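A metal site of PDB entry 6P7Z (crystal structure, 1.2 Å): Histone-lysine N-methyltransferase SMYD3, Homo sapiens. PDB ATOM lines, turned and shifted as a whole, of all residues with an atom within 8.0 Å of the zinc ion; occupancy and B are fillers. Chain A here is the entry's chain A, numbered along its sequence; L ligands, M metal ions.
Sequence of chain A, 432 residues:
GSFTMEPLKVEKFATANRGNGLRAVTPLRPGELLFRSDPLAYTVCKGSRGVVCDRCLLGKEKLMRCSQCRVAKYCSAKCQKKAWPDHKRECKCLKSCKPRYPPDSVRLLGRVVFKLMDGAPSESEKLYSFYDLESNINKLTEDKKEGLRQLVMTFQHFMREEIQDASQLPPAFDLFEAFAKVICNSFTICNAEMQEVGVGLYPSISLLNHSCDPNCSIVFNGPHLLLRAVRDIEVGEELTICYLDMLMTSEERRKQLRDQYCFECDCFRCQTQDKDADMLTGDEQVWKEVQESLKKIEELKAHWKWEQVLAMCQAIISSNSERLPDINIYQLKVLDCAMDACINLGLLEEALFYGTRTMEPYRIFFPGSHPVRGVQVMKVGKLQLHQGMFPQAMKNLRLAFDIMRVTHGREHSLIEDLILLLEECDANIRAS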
ATOM      1  N   HIS A 210      14.012   2.884 -14.612  1.00  0.00           N
ATOM      2  CA  HIS A 210      12.782   2.132 -14.749  1.00  0.00           C
ATOM      3  C   HIS A 210      12.982   0.845 -15.524  1.00  0.00           C
ATOM      4  O   HIS A 210      13.742   0.803 -16.512  1.00  0.00           O
ATOM      5  CB  HIS A 210      11.763   2.984 -15.519  1.00  0.00           C
ATOM      6  CG  HIS A 210      10.610   2.202 -16.028  1.00  0.00           C
ATOM      7  ND1 HIS A 210       9.493   1.917 -15.270  1.00  0.00           N
ATOM      8  CD2 HIS A 210      10.417   1.586 -17.228  1.00  0.00           C
ATOM      9  CE1 HIS A 210       8.654   1.192 -15.987  1.00  0.00           C
ATOM     10  NE2 HIS A 210       9.203   0.956 -17.167  1.00  0.00           N
ATOM     11  N   SER A 211      12.254  -0.185 -15.120  1.00  0.00           N
ATOM     12  CA  SER A 211      12.049  -1.369 -15.937  1.00  0.00           C
ATOM     13  C   SER A 211      10.617  -1.832 -15.792  1.00  0.00           C
ATOM     14  O   SER A 211      10.041  -1.754 -14.697  1.00  0.00           O
ATOM     15  CB  SER A 211      12.993  -2.495 -15.508  1.00  0.00           C
ATOM     16  OG  SER A 211      12.628  -3.688 -16.187  1.00  0.00           O
ATOM     17  N   CYS A 212      10.036  -2.340 -16.884  1.00  0.00           N
ATOM     18  CA  CYS A 212       8.720  -2.956 -16.851  1.00  0.00           C
ATOM     19  C   CYS A 212       8.745  -4.368 -16.252  1.00  0.00           C
ATOM     20  O   CYS A 212       7.686  -4.981 -16.097  1.00  0.00           O
ATOM     21  CB  CYS A 212       8.089  -2.983 -18.250  1.00  0.00           C
ATOM     22  SG  CYS A 212       8.088  -1.414 -19.123  1.00  0.00           S
ATOM     23  N   ASP A 213       9.942  -4.847 -15.899  1.00  0.00           N
ATOM     24  CA  ASP A 213      10.128  -6.116 -15.198  1.00  0.00           C
ATOM     25  C   ASP A 213      11.341  -5.948 -14.291  1.00  0.00           C
ATOM     26  O   ASP A 213      12.444  -6.383 -14.613  1.00  0.00           O
ATOM     27  CB  ASP A 213      10.329  -7.270 -16.185  1.00  0.00           C
ATOM     28  CG  ASP A 213      10.504  -8.608 -15.494  1.00  0.00           C
ATOM     29  OD1 ASP A 213      10.296  -8.708 -14.263  1.00  0.00           O
ATOM     30  OD2 ASP A 213      10.834  -9.586 -16.192  1.00  0.00           O
ATOM     31  N   CYS A 242       9.924  -0.474 -11.221  1.00  0.00           N
ATOM     32  CA  CYS A 242       8.898  -0.127 -12.195  1.00  0.00           C
ATOM     33  C   CYS A 242       8.221   1.163 -11.752  1.00  0.00           C
ATOM     34  O   CYS A 242       7.611   1.202 -10.682  1.00  0.00           O
ATOM     35  CB  CYS A 242       7.902  -1.262 -12.359  1.00  0.00           C
ATOM     36  SG  CYS A 242       6.724  -0.966 -13.712  1.00  0.00           S
ATOM     37  N   LEU A 244       5.630   2.419 -12.910  1.00  0.00           N
ATOM     38  CA  LEU A 244       4.235   2.456 -13.331  1.00  0.00           C
ATOM     39  C   LEU A 244       3.414   1.345 -12.701  1.00  0.00           C
ATOM     40  O   LEU A 244       3.926   0.270 -12.369  1.00  0.00           O
ATOM     41  CB  LEU A 244       4.150   2.279 -14.840  1.00  0.00           C
ATOM     42  CG  LEU A 244       4.971   3.239 -15.676  1.00  0.00           C
ATOM     43  CD1 LEU A 244       4.774   2.923 -17.147  1.00  0.00           C
ATOM     44  CD2 LEU A 244       4.527   4.643 -15.375  1.00  0.00           C
ATOM     45  N   SER A 250       1.332  -2.036 -23.044  1.00  0.00           N
ATOM     46  CA  SER A 250       2.575  -1.419 -23.510  1.00  0.00           C
ATOM     47  C   SER A 250       2.340  -0.059 -24.165  1.00  0.00           C
ATOM     48  O   SER A 250       3.192   0.823 -24.069  1.00  0.00           O
ATOM     49  CB  SER A 250       3.350  -2.344 -24.446  1.00  0.00           C
ATOM     50  OG  SER A 250       2.640  -2.600 -25.639  1.00  0.00           O
ATOM     51  N   ARG A 253       1.908   2.314 -21.228  1.00  0.00           N
ATOM     52  CA  ARG A 253       3.229   2.590 -20.667  1.00  0.00           C
ATOM     53  C   ARG A 253       4.016   3.514 -21.581  1.00  0.00           C
ATOM     54  O   ARG A 253       4.672   4.438 -21.101  1.00  0.00           O
ATOM     55  CB  ARG A 253       3.998   1.290 -20.411  1.00  0.00           C
ATOM     56  CG  ARG A 253       3.293   0.360 -19.440  1.00  0.00           C
ATOM     57  CD  ARG A 253       4.243  -0.684 -18.838  1.00  0.00           C
ATOM     58  NE  ARG A 253       4.924  -1.502 -19.837  1.00  0.00           N
ATOM     59  CZ  ARG A 253       4.393  -2.566 -20.440  1.00  0.00           C
ATOM     60  NH1 ARG A 253       3.144  -2.944 -20.162  1.00  0.00           N
ATOM     61  NH2 ARG A 253       5.117  -3.229 -21.326  1.00  0.00           N
ATOM     62  N   ARG A 254       3.953   3.296 -22.884  1.00  0.00           N
ATOM     63  CA  ARG A 254       4.700   4.157 -23.801  1.00  0.00           C
ATOM     64  C   ARG A 254       4.279   5.603 -23.631  1.00  0.00           C
ATOM     65  O   ARG A 254       5.124   6.516 -23.573  1.00  0.00           O
ATOM     66  CB  ARG A 254       4.486   3.706 -25.246  1.00  0.00           C
ATOM     67  CG  ARG A 254       5.050   4.694 -26.272  1.00  0.00           C
ATOM     68  CD  ARG A 254       5.007   4.128 -27.693  1.00  0.00           C
ATOM     69  NE  ARG A 254       5.842   2.939 -27.794  1.00  0.00           N
ATOM     70  CZ  ARG A 254       5.397   1.694 -27.916  1.00  0.00           C
ATOM     71  NH1 ARG A 254       4.097   1.453 -28.001  1.00  0.00           N
ATOM     72  NH2 ARG A 254       6.252   0.692 -27.954  1.00  0.00           N
ATOM     73  N   LEU A 257       5.549   6.948 -20.144  1.00  0.00           N
ATOM     74  CA  LEU A 257       7.005   7.094 -20.100  1.00  0.00           C
ATOM     75  C   LEU A 257       7.493   8.220 -21.002  1.00  0.00           C
ATOM     76  O   LEU A 257       8.444   8.927 -20.650  1.00  0.00           O
ATOM     77  CB  LEU A 257       7.689   5.767 -20.418  1.00  0.00           C
ATOM     78  CG  LEU A 257       7.393   4.635 -19.422  1.00  0.00           C
ATOM     79  CD1 LEU A 257       8.037   3.347 -19.888  1.00  0.00           C
ATOM     80  CD2 LEU A 257       7.840   4.980 -18.006  1.00  0.00           C
ATOM     81  N   PHE A 263      11.281   9.192 -22.101  1.00  0.00           N
ATOM     82  CA  PHE A 263      12.095   8.140 -22.709  1.00  0.00           C
ATOM     83  C   PHE A 263      11.222   7.093 -23.365  1.00  0.00           C
ATOM     84  O   PHE A 263      10.024   6.997 -23.110  1.00  0.00           O
ATOM     85  CB  PHE A 263      13.117   7.498 -21.764  1.00  0.00           C
ATOM     86  CG  PHE A 263      12.518   6.574 -20.734  1.00  0.00           C
ATOM     87  CD1 PHE A 263      12.053   7.073 -19.522  1.00  0.00           C
ATOM     88  CD2 PHE A 263      12.432   5.201 -20.961  1.00  0.00           C
ATOM     89  CE1 PHE A 263      11.523   6.222 -18.562  1.00  0.00           C
ATOM     90  CE2 PHE A 263      11.897   4.343 -19.996  1.00  0.00           C
ATOM     91  CZ  PHE A 263      11.437   4.865 -18.805  1.00  0.00           C
ATOM     92  N   GLU A 264      11.863   6.312 -24.252  1.00  0.00           N
ATOM     93  CA  GLU A 264      11.273   5.202 -24.986  1.00  0.00           C
ATOM     94  C   GLU A 264      11.817   3.912 -24.394  1.00  0.00           C
ATOM     95  O   GLU A 264      13.036   3.744 -24.277  1.00  0.00           O
ATOM     96  CB  GLU A 264      11.692   5.266 -26.466  1.00  0.00           C
ATOM     97  CG  GLU A 264      11.720   6.669 -27.072  1.00  0.00           C
ATOM     98  CD  GLU A 264      10.336   7.290 -27.180  1.00  0.00           C
ATOM     99  OE1 GLU A 264      10.250   8.508 -27.456  1.00  0.00           O
ATOM    100  OE2 GLU A 264       9.322   6.575 -26.996  1.00  0.00           O
ATOM    101  N   CYS A 265      10.935   3.021 -23.965  1.00  0.00           N
ATOM    102  CA  CYS A 265      11.364   1.821 -23.253  1.00  0.00           C
ATOM    103  C   CYS A 265      11.678   0.711 -24.237  1.00  0.00           C
ATOM    104  O   CYS A 265      10.837   0.362 -25.083  1.00  0.00           O
ATOM    105  CB  CYS A 265      10.328   1.306 -22.254  1.00  0.00           C
ATOM    106  SG  CYS A 265      10.950   0.056 -21.075  1.00  0.00           S
ATOM    107  N   ASP A 266      12.881   0.146 -24.109  1.00  0.00           N
ATOM    108  CA  ASP A 266      13.419  -0.880 -24.982  1.00  0.00           C
ATOM    109  C   ASP A 266      13.316  -2.293 -24.395  1.00  0.00           C
ATOM    110  O   ASP A 266      13.861  -3.230 -24.975  1.00  0.00           O
ATOM    111  CB  ASP A 266      14.874  -0.568 -25.350  1.00  0.00           C
ATOM    112  CG  ASP A 266      15.825  -0.634 -24.152  1.00  0.00           C
ATOM    113  OD1 ASP A 266      15.361  -0.713 -22.991  1.00  0.00           O
ATOM    114  OD2 ASP A 266      17.064  -0.620 -24.371  1.00  0.00           O
ATOM    115  N   CYS A 267      12.637  -2.462 -23.252  1.00  0.00           N
ATOM    116  CA  CYS A 267      12.650  -3.737 -22.552  1.00  0.00           C
ATOM    117  C   CYS A 267      11.918  -4.830 -23.361  1.00  0.00           C
ATOM    118  O   CYS A 267      11.200  -4.567 -24.326  1.00  0.00           O
ATOM    119  CB  CYS A 267      12.089  -3.586 -21.141  1.00  0.00           C
ATOM    120  SG  CYS A 267      10.311  -3.692 -21.040  1.00  0.00           S
ATOM    121  N   PHE A 268      12.166  -6.089 -22.971  1.00  0.00           N
ATOM    122  CA  PHE A 268      11.559  -7.214 -23.683  1.00  0.00           C
ATOM    123  C   PHE A 268      10.039  -7.118 -23.696  1.00  0.00           C
ATOM    124  O   PHE A 268       9.387  -7.452 -24.685  1.00  0.00           O
ATOM    125  CB  PHE A 268      12.000  -8.537 -23.070  1.00  0.00           C
ATOM    126  CG  PHE A 268      11.154  -9.712 -23.485  1.00  0.00           C
ATOM    127  CD1 PHE A 268      11.369 -10.329 -24.706  1.00  0.00           C
ATOM    128  CD2 PHE A 268      10.140 -10.182 -22.668  1.00  0.00           C
ATOM    129  CE1 PHE A 268      10.605 -11.402 -25.103  1.00  0.00           C
ATOM    130  CE2 PHE A 268       9.363 -11.262 -23.065  1.00  0.00           C
ATOM    131  CZ  PHE A 268       9.591 -11.872 -24.286  1.00  0.00           C
ATOM    132  N   ARG A 269       9.454  -6.672 -22.579  1.00  0.00           N
ATOM    133  CA  ARG A 269       8.001  -6.619 -22.502  1.00  0.00           C
ATOM    134  C   ARG A 269       7.447  -5.616 -23.510  1.00  0.00           C
ATOM    135  O   ARG A 269       6.436  -5.899 -24.161  1.00  0.00           O
ATOM    136  CB  ARG A 269       7.554  -6.260 -21.089  1.00  0.00           C
ATOM    137  CG  ARG A 269       7.898  -7.308 -20.033  1.00  0.00           C
ATOM    138  CD  ARG A 269       7.091  -7.089 -18.752  1.00  0.00           C
ATOM    139  NE  ARG A 269       5.665  -7.200 -19.043  1.00  0.00           N
ATOM    140  CZ  ARG A 269       4.728  -6.376 -18.582  1.00  0.00           C
ATOM    141  NH1 ARG A 269       5.031  -5.396 -17.736  1.00  0.00           N
ATOM    142  NH2 ARG A 269       3.472  -6.545 -18.962  1.00  0.00           N
ATOM    143  N   CYS A 270       8.089  -4.457 -23.640  1.00  0.00           N
ATOM    144  CA  CYS A 270       7.600  -3.459 -24.602  1.00  0.00           C
ATOM    145  C   CYS A 270       7.806  -3.921 -26.033  1.00  0.00           C
ATOM    146  O   CYS A 270       6.936  -3.744 -26.883  1.00  0.00           O
ATOM    147  CB  CYS A 270       8.257  -2.113 -24.316  1.00  0.00           C
ATOM    148  SG  CYS A 270       7.683  -1.447 -22.724  1.00  0.00           S
ATOM    149  N   GLN A 271       8.945  -4.566 -26.309  1.00  0.00           N
ATOM    150  CA  GLN A 271       9.208  -5.035 -27.666  1.00  0.00           C
ATOM    151  C   GLN A 271       8.207  -6.096 -28.109  1.00  0.00           C
ATOM    152  O   GLN A 271       7.904  -6.198 -29.302  1.00  0.00           O
ATOM    153  CB  GLN A 271      10.641  -5.596 -27.773  1.00  0.00           C
ATOM    154  CG  GLN A 271      11.770  -4.602 -27.466  1.00  0.00           C
ATOM    155  CD  GLN A 271      13.132  -5.278 -27.488  1.00  0.00           C
ATOM    156  OE1 GLN A 271      13.425  -6.096 -28.356  1.00  0.00           O
ATOM    157  NE2 GLN A 271      13.972  -4.951 -26.504  1.00  0.00           N
HETATM  158  N1  LIG L   1      18.637   8.442 -15.066  1.00  0.00           N
HETATM  159  C1  LIG L   1      18.169   9.370 -14.024  1.00  0.00           C
HETATM  160  C2  LIG L   1      19.212  10.437 -13.707  1.00  0.00           C
HETATM  161  O1  LIG L   1      19.011  11.212 -12.766  1.00  0.00           O
HETATM  162  O2  LIG L   1      20.225  10.490 -14.434  1.00  0.00           O
HETATM  163  C3  LIG L   1      17.719   8.606 -12.787  1.00  0.00           C
HETATM  164  C4  LIG L   1      16.266   8.123 -12.892  1.00  0.00           C
HETATM  165  S1  LIG L   1      15.112   9.527 -12.838  1.00  0.00           S
HETATM  166  C5  LIG L   1      13.955   9.056 -11.541  1.00  0.00           C
HETATM  167  C6  LIG L   1      14.076   9.258 -14.316  1.00  0.00           C
HETATM  168  C7  LIG L   1      14.745   9.565 -15.637  1.00  0.00           C
HETATM  169  O3  LIG L   1      15.736   8.592 -15.898  1.00  0.00           O
HETATM  170  C8  LIG L   1      13.796   9.474 -16.821  1.00  0.00           C
HETATM  171  O4  LIG L   1      13.055  10.666 -16.939  1.00  0.00           O
HETATM  172  C9  LIG L   1      14.760   9.191 -17.949  1.00  0.00           C
HETATM  173  O5  LIG L   1      15.478  10.386 -18.251  1.00  0.00           O
HETATM  174  C10 LIG L   1      15.714   8.242 -17.272  1.00  0.00           C
HETATM  175  N2  LIG L   1      15.310   6.823 -17.352  1.00  0.00           N
HETATM  176  C11 LIG L   1      14.767   6.068 -16.329  1.00  0.00           C
HETATM  177  N3  LIG L   1      14.563   4.811 -16.757  1.00  0.00           N
HETATM  178  C12 LIG L   1      14.973   4.744 -18.049  1.00  0.00           C
HETATM  179  C13 LIG L   1      15.000   3.722 -19.000  1.00  0.00           C
HETATM  180  N4  LIG L   1      14.590   2.462 -18.758  1.00  0.00           N
HETATM  181  N5  LIG L   1      15.492   3.996 -20.248  1.00  0.00           N
HETATM  182  C14 LIG L   1      15.931   5.267 -20.564  1.00  0.00           C
HETATM  183  N6  LIG L   1      15.912   6.291 -19.659  1.00  0.00           N
HETATM  184  C15 LIG L   1      15.444   6.003 -18.429  1.00  0.00           C
HETATM  185 ZN    ZN M   1       9.347  -1.624 -21.090  1.00  0.00          ZN
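The backbone NH (N) of His 210 is in hydrogen-bond range of a nitrogen (N3) of the ligand.
O of His 210 is in hydrogen-bond range of N4 of the ligand (2.9 Å).
The side-chain sulfur (SG) of Cys 267 sits close to the backbone NH (N) of Arg 269.
The guanidinium group of Arg 253 lies close to the side-chain sulfur of Cys 270 (3.4 Å).
The guanidinium group of Arg 253 lies close to the side-chain sulfur of Cys 212.
A ring nitrogen (NE2) of His 210 lies within hydrogen-bond range of the backbone NH of Cys 212, at 3.4 Å.
The guanidinium group (NH1) of Arg 269 sits at hydrogen-bond distance from the backbone carbonyl oxygen (O) of Cys 212.
The zinc ion is bound by the side-chain sulfur of Cys 267, the side-chain sulfur of Cys 265, the side-chain sulfur of Cys 270 and the side-chain sulfur of Cys 212.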
